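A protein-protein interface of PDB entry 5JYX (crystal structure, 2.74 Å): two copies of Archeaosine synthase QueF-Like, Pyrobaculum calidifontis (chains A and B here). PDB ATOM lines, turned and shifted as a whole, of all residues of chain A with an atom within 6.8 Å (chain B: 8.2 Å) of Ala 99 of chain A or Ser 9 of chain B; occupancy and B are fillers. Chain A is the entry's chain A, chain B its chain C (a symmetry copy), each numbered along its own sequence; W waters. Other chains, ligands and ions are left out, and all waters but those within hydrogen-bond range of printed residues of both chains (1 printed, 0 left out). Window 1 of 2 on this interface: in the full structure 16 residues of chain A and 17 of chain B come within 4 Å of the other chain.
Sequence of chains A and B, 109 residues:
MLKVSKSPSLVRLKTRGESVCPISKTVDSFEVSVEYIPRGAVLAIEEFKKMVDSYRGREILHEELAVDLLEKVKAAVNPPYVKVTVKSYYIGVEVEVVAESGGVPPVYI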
ATOM      1  N   GLU A  63      -8.018 -12.437   2.943  1.00  0.00           N
ATOM      2  CA  GLU A  63      -8.361 -12.817   4.304  1.00  0.00           C
ATOM      3  C   GLU A  63      -7.988 -11.661   5.220  1.00  0.00           C
ATOM      4  O   GLU A  63      -8.692 -11.367   6.162  1.00  0.00           O
ATOM      5  CB  GLU A  63      -7.603 -14.095   4.668  1.00  0.00           C
ATOM      6  CG  GLU A  63      -8.069 -15.358   3.900  1.00  0.00           C
ATOM      7  CD  GLU A  63      -7.390 -15.652   2.508  1.00  0.00           C
ATOM      8  OE1 GLU A  63      -6.729 -14.693   1.971  1.00  0.00           O
ATOM      9  OE2 GLU A  63      -7.525 -16.853   1.971  1.00  0.00           O
ATOM     10  N   LEU A  65      -7.762  -8.456   4.223  1.00  0.00           N
ATOM     11  CA  LEU A  65      -8.596  -7.347   3.854  1.00  0.00           C
ATOM     12  C   LEU A  65      -9.954  -7.383   4.594  1.00  0.00           C
ATOM     13  O   LEU A  65     -10.349  -6.427   5.244  1.00  0.00           O
ATOM     14  CB  LEU A  65      -8.737  -7.357   2.336  1.00  0.00           C
ATOM     15  CG  LEU A  65      -9.255  -6.112   1.662  1.00  0.00           C
ATOM     16  CD1 LEU A  65      -8.905  -6.087   0.186  1.00  0.00           C
ATOM     17  CD2 LEU A  65     -10.754  -6.013   1.808  1.00  0.00           C
ATOM     18  N   ALA A  66     -10.678  -8.498   4.510  1.00  0.00           N
ATOM     19  CA  ALA A  66     -11.936  -8.648   5.225  1.00  0.00           C
ATOM     20  C   ALA A  66     -11.753  -8.166   6.646  1.00  0.00           C
ATOM     21  O   ALA A  66     -12.554  -7.437   7.143  1.00  0.00           O
ATOM     22  CB  ALA A  66     -12.352 -10.083   5.224  1.00  0.00           C
ATOM     23  N   VAL A  67     -10.649  -8.536   7.270  1.00  0.00           N
ATOM     24  CA  VAL A  67     -10.360  -8.210   8.648  1.00  0.00           C
ATOM     25  C   VAL A  67      -9.875  -6.792   8.791  1.00  0.00           C
ATOM     26  O   VAL A  67     -10.247  -6.124   9.723  1.00  0.00           O
ATOM     27  CB  VAL A  67      -9.321  -9.210   9.223  1.00  0.00           C
ATOM     28  CG1 VAL A  67      -8.629  -8.723  10.479  1.00  0.00           C
ATOM     29  CG2 VAL A  67     -10.015 -10.520   9.543  1.00  0.00           C
ATOM     30  N   ASP A  68      -9.051  -6.310   7.891  1.00  0.00           N
ATOM     31  CA  ASP A  68      -8.685  -4.907   7.966  1.00  0.00           C
ATOM     32  C   ASP A  68      -9.900  -3.972   7.909  1.00  0.00           C
ATOM     33  O   ASP A  68      -9.972  -2.976   8.615  1.00  0.00           O
ATOM     34  CB  ASP A  68      -7.744  -4.564   6.851  1.00  0.00           C
ATOM     35  CG  ASP A  68      -7.181  -3.175   6.993  1.00  0.00           C
ATOM     36  OD1 ASP A  68      -6.129  -3.074   7.654  1.00  0.00           O
ATOM     37  OD2 ASP A  68      -7.764  -2.185   6.477  1.00  0.00           O
ATOM     38  N   LEU A  70     -13.073  -4.687   8.431  1.00  0.00           N
ATOM     39  CA  LEU A  70     -13.890  -4.868   9.613  1.00  0.00           C
ATOM     40  C   LEU A  70     -13.478  -3.914  10.710  1.00  0.00           C
ATOM     41  O   LEU A  70     -14.316  -3.305  11.339  1.00  0.00           O
ATOM     42  CB  LEU A  70     -13.750  -6.277  10.153  1.00  0.00           C
ATOM     43  CG  LEU A  70     -14.594  -6.592  11.414  1.00  0.00           C
ATOM     44  CD1 LEU A  70     -16.060  -6.740  11.081  1.00  0.00           C
ATOM     45  CD2 LEU A  70     -14.116  -7.901  11.972  1.00  0.00           C
ATOM     46  N   TYR A  81     -22.849  -5.002  15.810  1.00  0.00           N
ATOM     47  CA  TYR A  81     -22.610  -6.158  14.941  1.00  0.00           C
ATOM     48  C   TYR A  81     -22.141  -5.782  13.575  1.00  0.00           C
ATOM     49  O   TYR A  81     -22.770  -4.930  12.951  1.00  0.00           O
ATOM     50  CB  TYR A  81     -23.877  -6.968  14.775  1.00  0.00           C
ATOM     51  CG  TYR A  81     -23.723  -8.082  13.756  1.00  0.00           C
ATOM     52  CD1 TYR A  81     -23.164  -9.289  14.103  1.00  0.00           C
ATOM     53  CD2 TYR A  81     -24.128  -7.896  12.433  1.00  0.00           C
ATOM     54  CE1 TYR A  81     -23.002 -10.291  13.176  1.00  0.00           C
ATOM     55  CE2 TYR A  81     -23.991  -8.898  11.497  1.00  0.00           C
ATOM     56  CZ  TYR A  81     -23.427 -10.102  11.876  1.00  0.00           C
ATOM     57  OH  TYR A  81     -23.341 -11.119  10.950  1.00  0.00           O
ATOM     58  N   VAL A  82     -21.080  -6.435  13.100  1.00  0.00           N
ATOM     59  CA  VAL A  82     -20.560  -6.145  11.762  1.00  0.00           C
ATOM     60  C   VAL A  82     -20.086  -7.378  11.048  1.00  0.00           C
ATOM     61  O   VAL A  82     -19.315  -8.149  11.610  1.00  0.00           O
ATOM     62  CB  VAL A  82     -19.367  -5.187  11.770  1.00  0.00           C
ATOM     63  CG1 VAL A  82     -19.110  -4.690  10.345  1.00  0.00           C
ATOM     64  CG2 VAL A  82     -19.646  -3.959  12.589  1.00  0.00           C
ATOM     65  N   LYS A  83     -20.497  -7.532   9.795  1.00  0.00           N
ATOM     66  CA  LYS A  83     -20.027  -8.641   8.959  1.00  0.00           C
ATOM     67  C   LYS A  83     -19.498  -8.139   7.626  1.00  0.00           C
ATOM     68  O   LYS A  83     -20.206  -7.518   6.849  1.00  0.00           O
ATOM     69  CB  LYS A  83     -21.142  -9.651   8.705  1.00  0.00           C
ATOM     70  CG  LYS A  83     -20.648 -10.923   8.017  1.00  0.00           C
ATOM     71  CD  LYS A  83     -21.694 -12.033   7.946  1.00  0.00           C
ATOM     72  CE  LYS A  83     -22.947 -11.576   7.207  1.00  0.00           C
ATOM     73  NZ  LYS A  83     -23.738 -12.717   6.632  1.00  0.00           N
ATOM     74  N   VAL A  84     -18.251  -8.436   7.366  1.00  0.00           N
ATOM     75  CA  VAL A  84     -17.600  -8.050   6.144  1.00  0.00           C
ATOM     76  C   VAL A  84     -17.426  -9.275   5.313  1.00  0.00           C
ATOM     77  O   VAL A  84     -16.947 -10.270   5.818  1.00  0.00           O
ATOM     78  CB  VAL A  84     -16.249  -7.502   6.447  1.00  0.00           C
ATOM     79  CG1 VAL A  84     -15.474  -7.272   5.150  1.00  0.00           C
ATOM     80  CG2 VAL A  84     -16.404  -6.236   7.296  1.00  0.00           C
ATOM     81  N   THR A  85     -17.854  -9.219   4.049  1.00  0.00           N
ATOM     82  CA  THR A  85     -17.632 -10.325   3.085  1.00  0.00           C
ATOM     83  C   THR A  85     -16.886  -9.860   1.869  1.00  0.00           C
ATOM     84  O   THR A  85     -17.375  -8.972   1.215  1.00  0.00           O
ATOM     85  CB  THR A  85     -18.934 -10.920   2.581  1.00  0.00           C
ATOM     86  OG1 THR A  85     -19.740 -11.264   3.697  1.00  0.00           O
ATOM     87  CG2 THR A  85     -18.655 -12.168   1.787  1.00  0.00           C
ATOM     88  N   VAL A  86     -15.734 -10.478   1.593  1.00  0.00           N
ATOM     89  CA  VAL A  86     -14.900 -10.235   0.401  1.00  0.00           C
ATOM     90  C   VAL A  86     -15.049 -11.429  -0.524  1.00  0.00           C
ATOM     91  O   VAL A  86     -15.072 -12.525  -0.040  1.00  0.00           O
ATOM     92  CB  VAL A  86     -13.429 -10.090   0.803  1.00  0.00           C
ATOM     93  CG1 VAL A  86     -12.524  -9.889  -0.427  1.00  0.00           C
ATOM     94  CG2 VAL A  86     -13.273  -8.945   1.782  1.00  0.00           C
ATOM     95  N   VAL A  97     -14.229 -14.680   1.741  1.00  0.00           N
ATOM     96  CA  VAL A  97     -13.827 -14.533   3.145  1.00  0.00           C
ATOM     97  C   VAL A  97     -14.929 -13.818   3.926  1.00  0.00           C
ATOM     98  O   VAL A  97     -15.534 -12.885   3.394  1.00  0.00           O
ATOM     99  CB  VAL A  97     -12.571 -13.719   3.245  1.00  0.00           C
ATOM    100  CG1 VAL A  97     -12.083 -13.792   4.668  1.00  0.00           C
ATOM    101  CG2 VAL A  97     -11.517 -14.258   2.301  1.00  0.00           C
ATOM    102  N   VAL A  98     -15.217 -14.250   5.147  1.00  0.00           N
ATOM    103  CA  VAL A  98     -16.161 -13.531   6.000  1.00  0.00           C
ATOM    104  C   VAL A  98     -15.500 -13.164   7.305  1.00  0.00           C
ATOM    105  O   VAL A  98     -14.792 -13.980   7.900  1.00  0.00           O
ATOM    106  CB  VAL A  98     -17.414 -14.352   6.308  1.00  0.00           C
ATOM    107  CG1 VAL A  98     -18.409 -13.539   7.087  1.00  0.00           C
ATOM    108  CG2 VAL A  98     -18.083 -14.800   5.043  1.00  0.00           C
ATOM    109  N   ALA A  99     -15.740 -11.946   7.787  1.00  0.00           N
ATOM    110  CA  ALA A  99     -15.239 -11.534   9.098  1.00  0.00           C
ATOM    111  C   ALA A  99     -16.368 -10.921   9.862  1.00  0.00           C
ATOM    112  O   ALA A  99     -17.122 -10.153   9.330  1.00  0.00           O
ATOM    113  CB  ALA A  99     -14.104 -10.570   8.916  1.00  0.00           C
ATOM    114  N   GLU A 100     -16.495 -11.303  11.124  1.00  0.00           N
ATOM    115  CA  GLU A 100     -17.623 -10.943  12.008  1.00  0.00           C
ATOM    116  C   GLU A 100     -17.174 -10.478  13.382  1.00  0.00           C
ATOM    117  O   GLU A 100     -16.140 -10.904  13.862  1.00  0.00           O
ATOM    118  CB  GLU A 100     -18.433 -12.191  12.281  1.00  0.00           C
ATOM    119  CG  GLU A 100     -19.442 -12.524  11.216  1.00  0.00           C
ATOM    120  CD  GLU A 100     -20.497 -13.460  11.758  1.00  0.00           C
ATOM    121  OE1 GLU A 100     -21.673 -13.035  11.866  1.00  0.00           O
ATOM    122  OE2 GLU A 100     -20.109 -14.593  12.144  1.00  0.00           O
ATOM    123  N   SER A 101     -18.022  -9.695  14.041  1.00  0.00           N
ATOM    124  CA  SER A 101     -17.742  -9.140  15.338  1.00  0.00           C
ATOM    125  C   SER A 101     -19.033  -8.768  15.993  1.00  0.00           C
ATOM    126  O   SER A 101     -19.807  -8.108  15.370  1.00  0.00           O
ATOM    127  CB  SER A 101     -16.886  -7.888  15.125  1.00  0.00           C
ATOM    128  OG  SER A 101     -16.591  -7.204  16.338  1.00  0.00           O
ATOM    129  N   LYS B   6      -5.100 -11.551  12.905  1.00  0.00           N
ATOM    130  CA  LYS B   6      -6.471 -11.938  13.215  1.00  0.00           C
ATOM    131  C   LYS B   6      -7.026 -12.800  12.063  1.00  0.00           C
ATOM    132  O   LYS B   6      -6.986 -12.425  10.885  1.00  0.00           O
ATOM    133  CB  LYS B   6      -7.384 -10.741  13.513  1.00  0.00           C
ATOM    134  CG  LYS B   6      -7.226 -10.094  14.896  1.00  0.00           C
ATOM    135  CD  LYS B   6      -8.549  -9.868  15.683  1.00  0.00           C
ATOM    136  CE  LYS B   6      -9.758  -9.262  14.901  1.00  0.00           C
ATOM    137  NZ  LYS B   6      -9.908  -7.765  14.798  1.00  0.00           N
ATOM    138  N   SER B   7      -7.534 -13.966  12.432  1.00  0.00           N
ATOM    139  CA  SER B   7      -8.099 -14.915  11.492  1.00  0.00           C
ATOM    140  C   SER B   7      -9.489 -14.402  11.074  1.00  0.00           C
ATOM    141  O   SER B   7     -10.126 -13.755  11.871  1.00  0.00           O
ATOM    142  CB  SER B   7      -8.191 -16.317  12.155  1.00  0.00           C
ATOM    143  OG  SER B   7      -6.958 -17.071  12.097  1.00  0.00           O
ATOM    144  N   PRO B   8      -9.947 -14.661   9.828  1.00  0.00           N
ATOM    145  CA  PRO B   8     -11.321 -14.383   9.485  1.00  0.00           C
ATOM    146  C   PRO B   8     -12.191 -15.396  10.132  1.00  0.00           C
ATOM    147  O   PRO B   8     -11.670 -16.257  10.738  1.00  0.00           O
ATOM    148  CB  PRO B   8     -11.356 -14.556   7.951  1.00  0.00           C
ATOM    149  CG  PRO B   8      -9.967 -14.484   7.487  1.00  0.00           C
ATOM    150  CD  PRO B   8      -9.185 -15.053   8.632  1.00  0.00           C
ATOM    151  N   SER B   9     -13.498 -15.291   9.993  1.00  0.00           N
ATOM    152  CA  SER B   9     -14.437 -16.194  10.621  1.00  0.00           C
ATOM    153  C   SER B   9     -14.673 -17.393   9.789  1.00  0.00           C
ATOM    154  O   SER B   9     -15.011 -18.443  10.321  1.00  0.00           O
ATOM    155  CB  SER B   9     -15.812 -15.552  10.751  1.00  0.00           C
ATOM    156  OG  SER B   9     -15.748 -14.290  11.366  1.00  0.00           O
ATOM    157  N   LEU B  10     -14.632 -17.210   8.463  1.00  0.00           N
ATOM    158  CA  LEU B  10     -15.014 -18.246   7.500  1.00  0.00           C
ATOM    159  C   LEU B  10     -14.300 -17.990   6.157  1.00  0.00           C
ATOM    160  O   LEU B  10     -14.182 -16.847   5.772  1.00  0.00           O
ATOM    161  CB  LEU B  10     -16.523 -18.190   7.335  1.00  0.00           C
ATOM    162  CG  LEU B  10     -17.202 -19.314   6.552  1.00  0.00           C
ATOM    163  CD1 LEU B  10     -17.094 -20.587   7.323  1.00  0.00           C
ATOM    164  CD2 LEU B  10     -18.657 -19.039   6.349  1.00  0.00           C
ATOM    165  N   VAL B  11     -13.796 -19.034   5.491  1.00  0.00           N
ATOM    166  CA  VAL B  11     -13.253 -18.976   4.109  1.00  0.00           C
ATOM    167  C   VAL B  11     -13.856 -20.088   3.278  1.00  0.00           C
ATOM    168  O   VAL B  11     -13.914 -21.207   3.753  1.00  0.00           O
ATOM    169  CB  VAL B  11     -11.714 -19.164   4.078  1.00  0.00           C
ATOM    170  CG1 VAL B  11     -11.157 -19.251   2.661  1.00  0.00           C
ATOM    171  CG2 VAL B  11     -11.046 -18.001   4.785  1.00  0.00           C
ATOM    172  N   ARG B  12     -14.355 -19.767   2.079  1.00  0.00           N
ATOM    173  CA  ARG B  12     -14.725 -20.764   1.085  1.00  0.00           C
ATOM    174  C   ARG B  12     -13.737 -20.603  -0.063  1.00  0.00           C
ATOM    175  O   ARG B  12     -13.385 -19.478  -0.441  1.00  0.00           O
ATOM    176  CB  ARG B  12     -16.159 -20.612   0.555  1.00  0.00           C
ATOM    177  CG  ARG B  12     -17.225 -20.411   1.620  1.00  0.00           C
ATOM    178  CD  ARG B  12     -18.646 -20.295   1.049  1.00  0.00           C
ATOM    179  NE  ARG B  12     -19.680 -20.087   2.087  1.00  0.00           N
ATOM    180  CZ  ARG B  12     -19.982 -18.931   2.712  1.00  0.00           C
ATOM    181  NH1 ARG B  12     -19.343 -17.772   2.486  1.00  0.00           N
ATOM    182  NH2 ARG B  12     -20.941 -18.936   3.622  1.00  0.00           N
ATOM    183  N   GLU B  35     -15.068 -25.178   2.677  1.00  0.00           N
ATOM    184  CA  GLU B  35     -15.429 -24.090   3.548  1.00  0.00           C
ATOM    185  C   GLU B  35     -14.835 -24.392   4.924  1.00  0.00           C
ATOM    186  O   GLU B  35     -14.941 -25.491   5.378  1.00  0.00           O
ATOM    187  CB  GLU B  35     -16.948 -23.992   3.532  1.00  0.00           C
ATOM    188  CG  GLU B  35     -17.635 -23.351   4.708  1.00  0.00           C
ATOM    189  CD  GLU B  35     -19.145 -23.275   4.480  1.00  0.00           C
ATOM    190  OE1 GLU B  35     -19.594 -23.043   3.299  1.00  0.00           O
ATOM    191  OE2 GLU B  35     -19.860 -23.485   5.498  1.00  0.00           O
ATOM    192  N   TYR B  36     -14.169 -23.455   5.563  1.00  0.00           N
ATOM    193  CA  TYR B  36     -13.396 -23.789   6.764  1.00  0.00           C
ATOM    194  C   TYR B  36     -13.253 -22.606   7.698  1.00  0.00           C
ATOM    195  O   TYR B  36     -13.233 -21.453   7.242  1.00  0.00           O
ATOM    196  CB  TYR B  36     -12.034 -24.411   6.406  1.00  0.00           C
ATOM    197  CG  TYR B  36     -10.932 -23.438   5.920  1.00  0.00           C
ATOM    198  CD1 TYR B  36     -10.803 -23.078   4.571  1.00  0.00           C
ATOM    199  CD2 TYR B  36     -10.018 -22.901   6.810  1.00  0.00           C
ATOM    200  CE1 TYR B  36      -9.821 -22.212   4.136  1.00  0.00           C
ATOM    201  CE2 TYR B  36      -9.027 -22.032   6.380  1.00  0.00           C
ATOM    202  CZ  TYR B  36      -8.934 -21.688   5.041  1.00  0.00           C
ATOM    203  OH  TYR B  36      -7.932 -20.819   4.661  1.00  0.00           O
ATOM    204  N   ILE B  37     -13.222 -22.873   9.006  1.00  0.00           N
ATOM    205  CA  ILE B  37     -13.001 -21.806   9.995  1.00  0.00           C
ATOM    206  C   ILE B  37     -11.509 -21.712  10.276  1.00  0.00           C
ATOM    207  O   ILE B  37     -10.925 -22.643  10.746  1.00  0.00           O
ATOM    208  CB  ILE B  37     -13.765 -22.045  11.285  1.00  0.00           C
ATOM    209  CG1 ILE B  37     -15.273 -22.083  11.015  1.00  0.00           C
ATOM    210  CG2 ILE B  37     -13.452 -20.953  12.254  1.00  0.00           C
ATOM    211  CD1 ILE B  37     -16.187 -22.196  12.243  1.00  0.00           C
ATOM    212  N   PRO B  38     -10.871 -20.606   9.960  1.00  0.00           N
ATOM    213  CA  PRO B  38      -9.447 -20.597  10.239  1.00  0.00           C
ATOM    214  C   PRO B  38      -9.078 -20.525  11.726  1.00  0.00           C
ATOM    215  O   PRO B  38      -9.856 -20.031  12.517  1.00  0.00           O
ATOM    216  CB  PRO B  38      -8.979 -19.331   9.537  1.00  0.00           C
ATOM    217  CG  PRO B  38      -9.932 -19.138   8.437  1.00  0.00           C
ATOM    218  CD  PRO B  38     -11.247 -19.523   9.042  1.00  0.00           C
ATOM    219  N   ARG B  39      -7.899 -21.049  12.065  1.00  0.00           N
ATOM    220  CA  ARG B  39      -7.245 -20.858  13.378  1.00  0.00           C
ATOM    221  C   ARG B  39      -5.745 -20.524  13.180  1.00  0.00           C
ATOM    222  O   ARG B  39      -4.943 -21.392  12.914  1.00  0.00           O
ATOM    223  CB  ARG B  39      -7.414 -22.116  14.222  1.00  0.00           C
ATOM    224  CG  ARG B  39      -7.995 -21.857  15.609  1.00  0.00           C
ATOM    225  CD  ARG B  39      -7.844 -23.079  16.524  1.00  0.00           C
ATOM    226  NE  ARG B  39      -7.902 -24.364  15.796  1.00  0.00           N
ATOM    227  CZ  ARG B  39      -7.932 -25.561  16.369  1.00  0.00           C
ATOM    228  NH1 ARG B  39      -7.904 -25.674  17.693  1.00  0.00           N
ATOM    229  NH2 ARG B  39      -8.004 -26.649  15.596  1.00  0.00           N
ATOM    230  N   PRO B  80     -10.929 -25.961  13.188  1.00  0.00           N
ATOM    231  CA  PRO B  80     -11.962 -26.631  13.991  1.00  0.00           C
ATOM    232  C   PRO B  80     -13.256 -27.017  13.231  1.00  0.00           C
ATOM    233  O   PRO B  80     -14.023 -27.777  13.733  1.00  0.00           O
ATOM    234  CB  PRO B  80     -12.265 -25.595  15.065  1.00  0.00           C
ATOM    235  CG  PRO B  80     -12.025 -24.298  14.406  1.00  0.00           C
ATOM    236  CD  PRO B  80     -10.893 -24.517  13.461  1.00  0.00           C
ATOM    237  N   TYR B  81     -13.512 -26.452  12.052  1.00  0.00           N
ATOM    238  CA  TYR B  81     -14.620 -26.901  11.170  1.00  0.00           C
ATOM    239  C   TYR B  81     -14.180 -26.907   9.700  1.00  0.00           C
ATOM    240  O   TYR B  81     -13.533 -26.009   9.280  1.00  0.00           O
ATOM    241  CB  TYR B  81     -15.848 -26.003  11.353  1.00  0.00           C
ATOM    242  CG  TYR B  81     -16.973 -26.296  10.407  1.00  0.00           C
ATOM    243  CD1 TYR B  81     -17.833 -27.349  10.615  1.00  0.00           C
ATOM    244  CD2 TYR B  81     -17.159 -25.527   9.280  1.00  0.00           C
ATOM    245  CE1 TYR B  81     -18.853 -27.612   9.740  1.00  0.00           C
ATOM    246  CE2 TYR B  81     -18.178 -25.789   8.398  1.00  0.00           C
ATOM    247  CZ  TYR B  81     -19.021 -26.825   8.647  1.00  0.00           C
ATOM    248  OH  TYR B  81     -20.025 -27.049   7.735  1.00  0.00           O
ATOM    249  N   VAL B 104     -19.832 -26.406  13.829  1.00  0.00           N
ATOM    250  CA  VAL B 104     -20.327 -25.161  13.190  1.00  0.00           C
ATOM    251  C   VAL B 104     -20.210 -23.931  14.118  1.00  0.00           C
ATOM    252  O   VAL B 104     -20.254 -22.784  13.659  1.00  0.00           O
ATOM    253  CB  VAL B 104     -21.800 -25.304  12.660  1.00  0.00           C
ATOM    254  CG1 VAL B 104     -21.976 -26.580  11.829  1.00  0.00           C
ATOM    255  CG2 VAL B 104     -22.833 -25.249  13.793  1.00  0.00           C
HETATM  256  O   HOH W   1      -7.711 -19.933   2.425  1.00  0.00           O
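Glu 63 of chain A touches Pro 8 of chain B (O to CG, 3.6 Å). Lys 6 of chain B touches Val 67 of chain A (O to CG2, 3.8 Å). Val 67 of chain A touches Ser 7 of chain B. CG1 of Val 97 of chain A touches CB of Pro 8 of chain B (3.4 Å). Leu 10 of chain B touches Val 97 of chain A (O to CA, 3.5 Å). CB of Pro 8 of chain B touches O of Val 98 of chain A, at 3.5 Å. OG of Ser 9 of chain B touches CA of Ala 99 of chain A, at 3.6 Å.
OE1 of Glu 100 of chain A lies within hydrogen-bond range of OH of Tyr 81 of chain A (2.7 Å). N of Val 84 of chain A sits at hydrogen-bond distance from O of Ala 99 of chain A. The backbone carbonyl oxygen (O) of Val 86 of chain A lies within hydrogen-bond range of the backbone NH (N) of Val 97 of chain A (2.9 Å).
O of Val 98 of chain A is in hydrogen-bond range of N of Ser 9 of chain B (2.8 Å). The backbone NH of Val 98 of chain A sits at hydrogen-bond distance from the backbone carbonyl oxygen of Leu 10 of chain B (2.9 Å). The side-chain hydroxyl of Ser 9 of chain B is in hydrogen-bond range of the backbone NH of Glu 100 of chain A, 3.1 Å away.
Position printed for both chains: 81. Of the 10 pairs that touch across the chains among the printed residues, none has its exchanged pair printed and touching as well.
Water W1 lies within hydrogen-bond range of the side-chain hydroxyl of Tyr 36 of chain B and the side-chain carboxylate of Glu 63 of chain A.
Of the 15 printed residues of chain B, 5 touch a printed residue of chain A. Printed residues of chain B that touch a printed residue of chain A: Lys 6, Ser 7, Pro 8, Ser 9 and Leu 10. Hydrophobic or aromatic side chains of chain B that line the printed part of chain A: Pro 8. Of the 17 printed residues of chain A, 6 touch a printed residue of chain B. Among the printed residues, 10 pairs touch across the chains.
Ala 99 of chain A touches just one residue of chain B: Ser 9 (3.6 Å). Ser 9 of chain B touches just these residues of chain A: Val 98, Ala 99 and Glu 100. Printed residues of chain B within 4 Å of Val 98 of chain A: Pro 8 (3.5 Å), Ser 9 (2.8 Å) and Leu 10 (2.9 Å). Printed residues of chain A within 4 Å of Pro 8 of chain B: Glu 63, Val 97 and Val 98. Of the printed residues of chain B, Glu 100 of chain A touches Ser 9. Ile 37 of chain B touches none of the printed residues of chain A. Glu 35 of chain B touches none of the printed residues of chain A. The nearest residue of chain B that does not touch Ala 99 of chain A is Pro 8 of chain B (4.8 Å).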
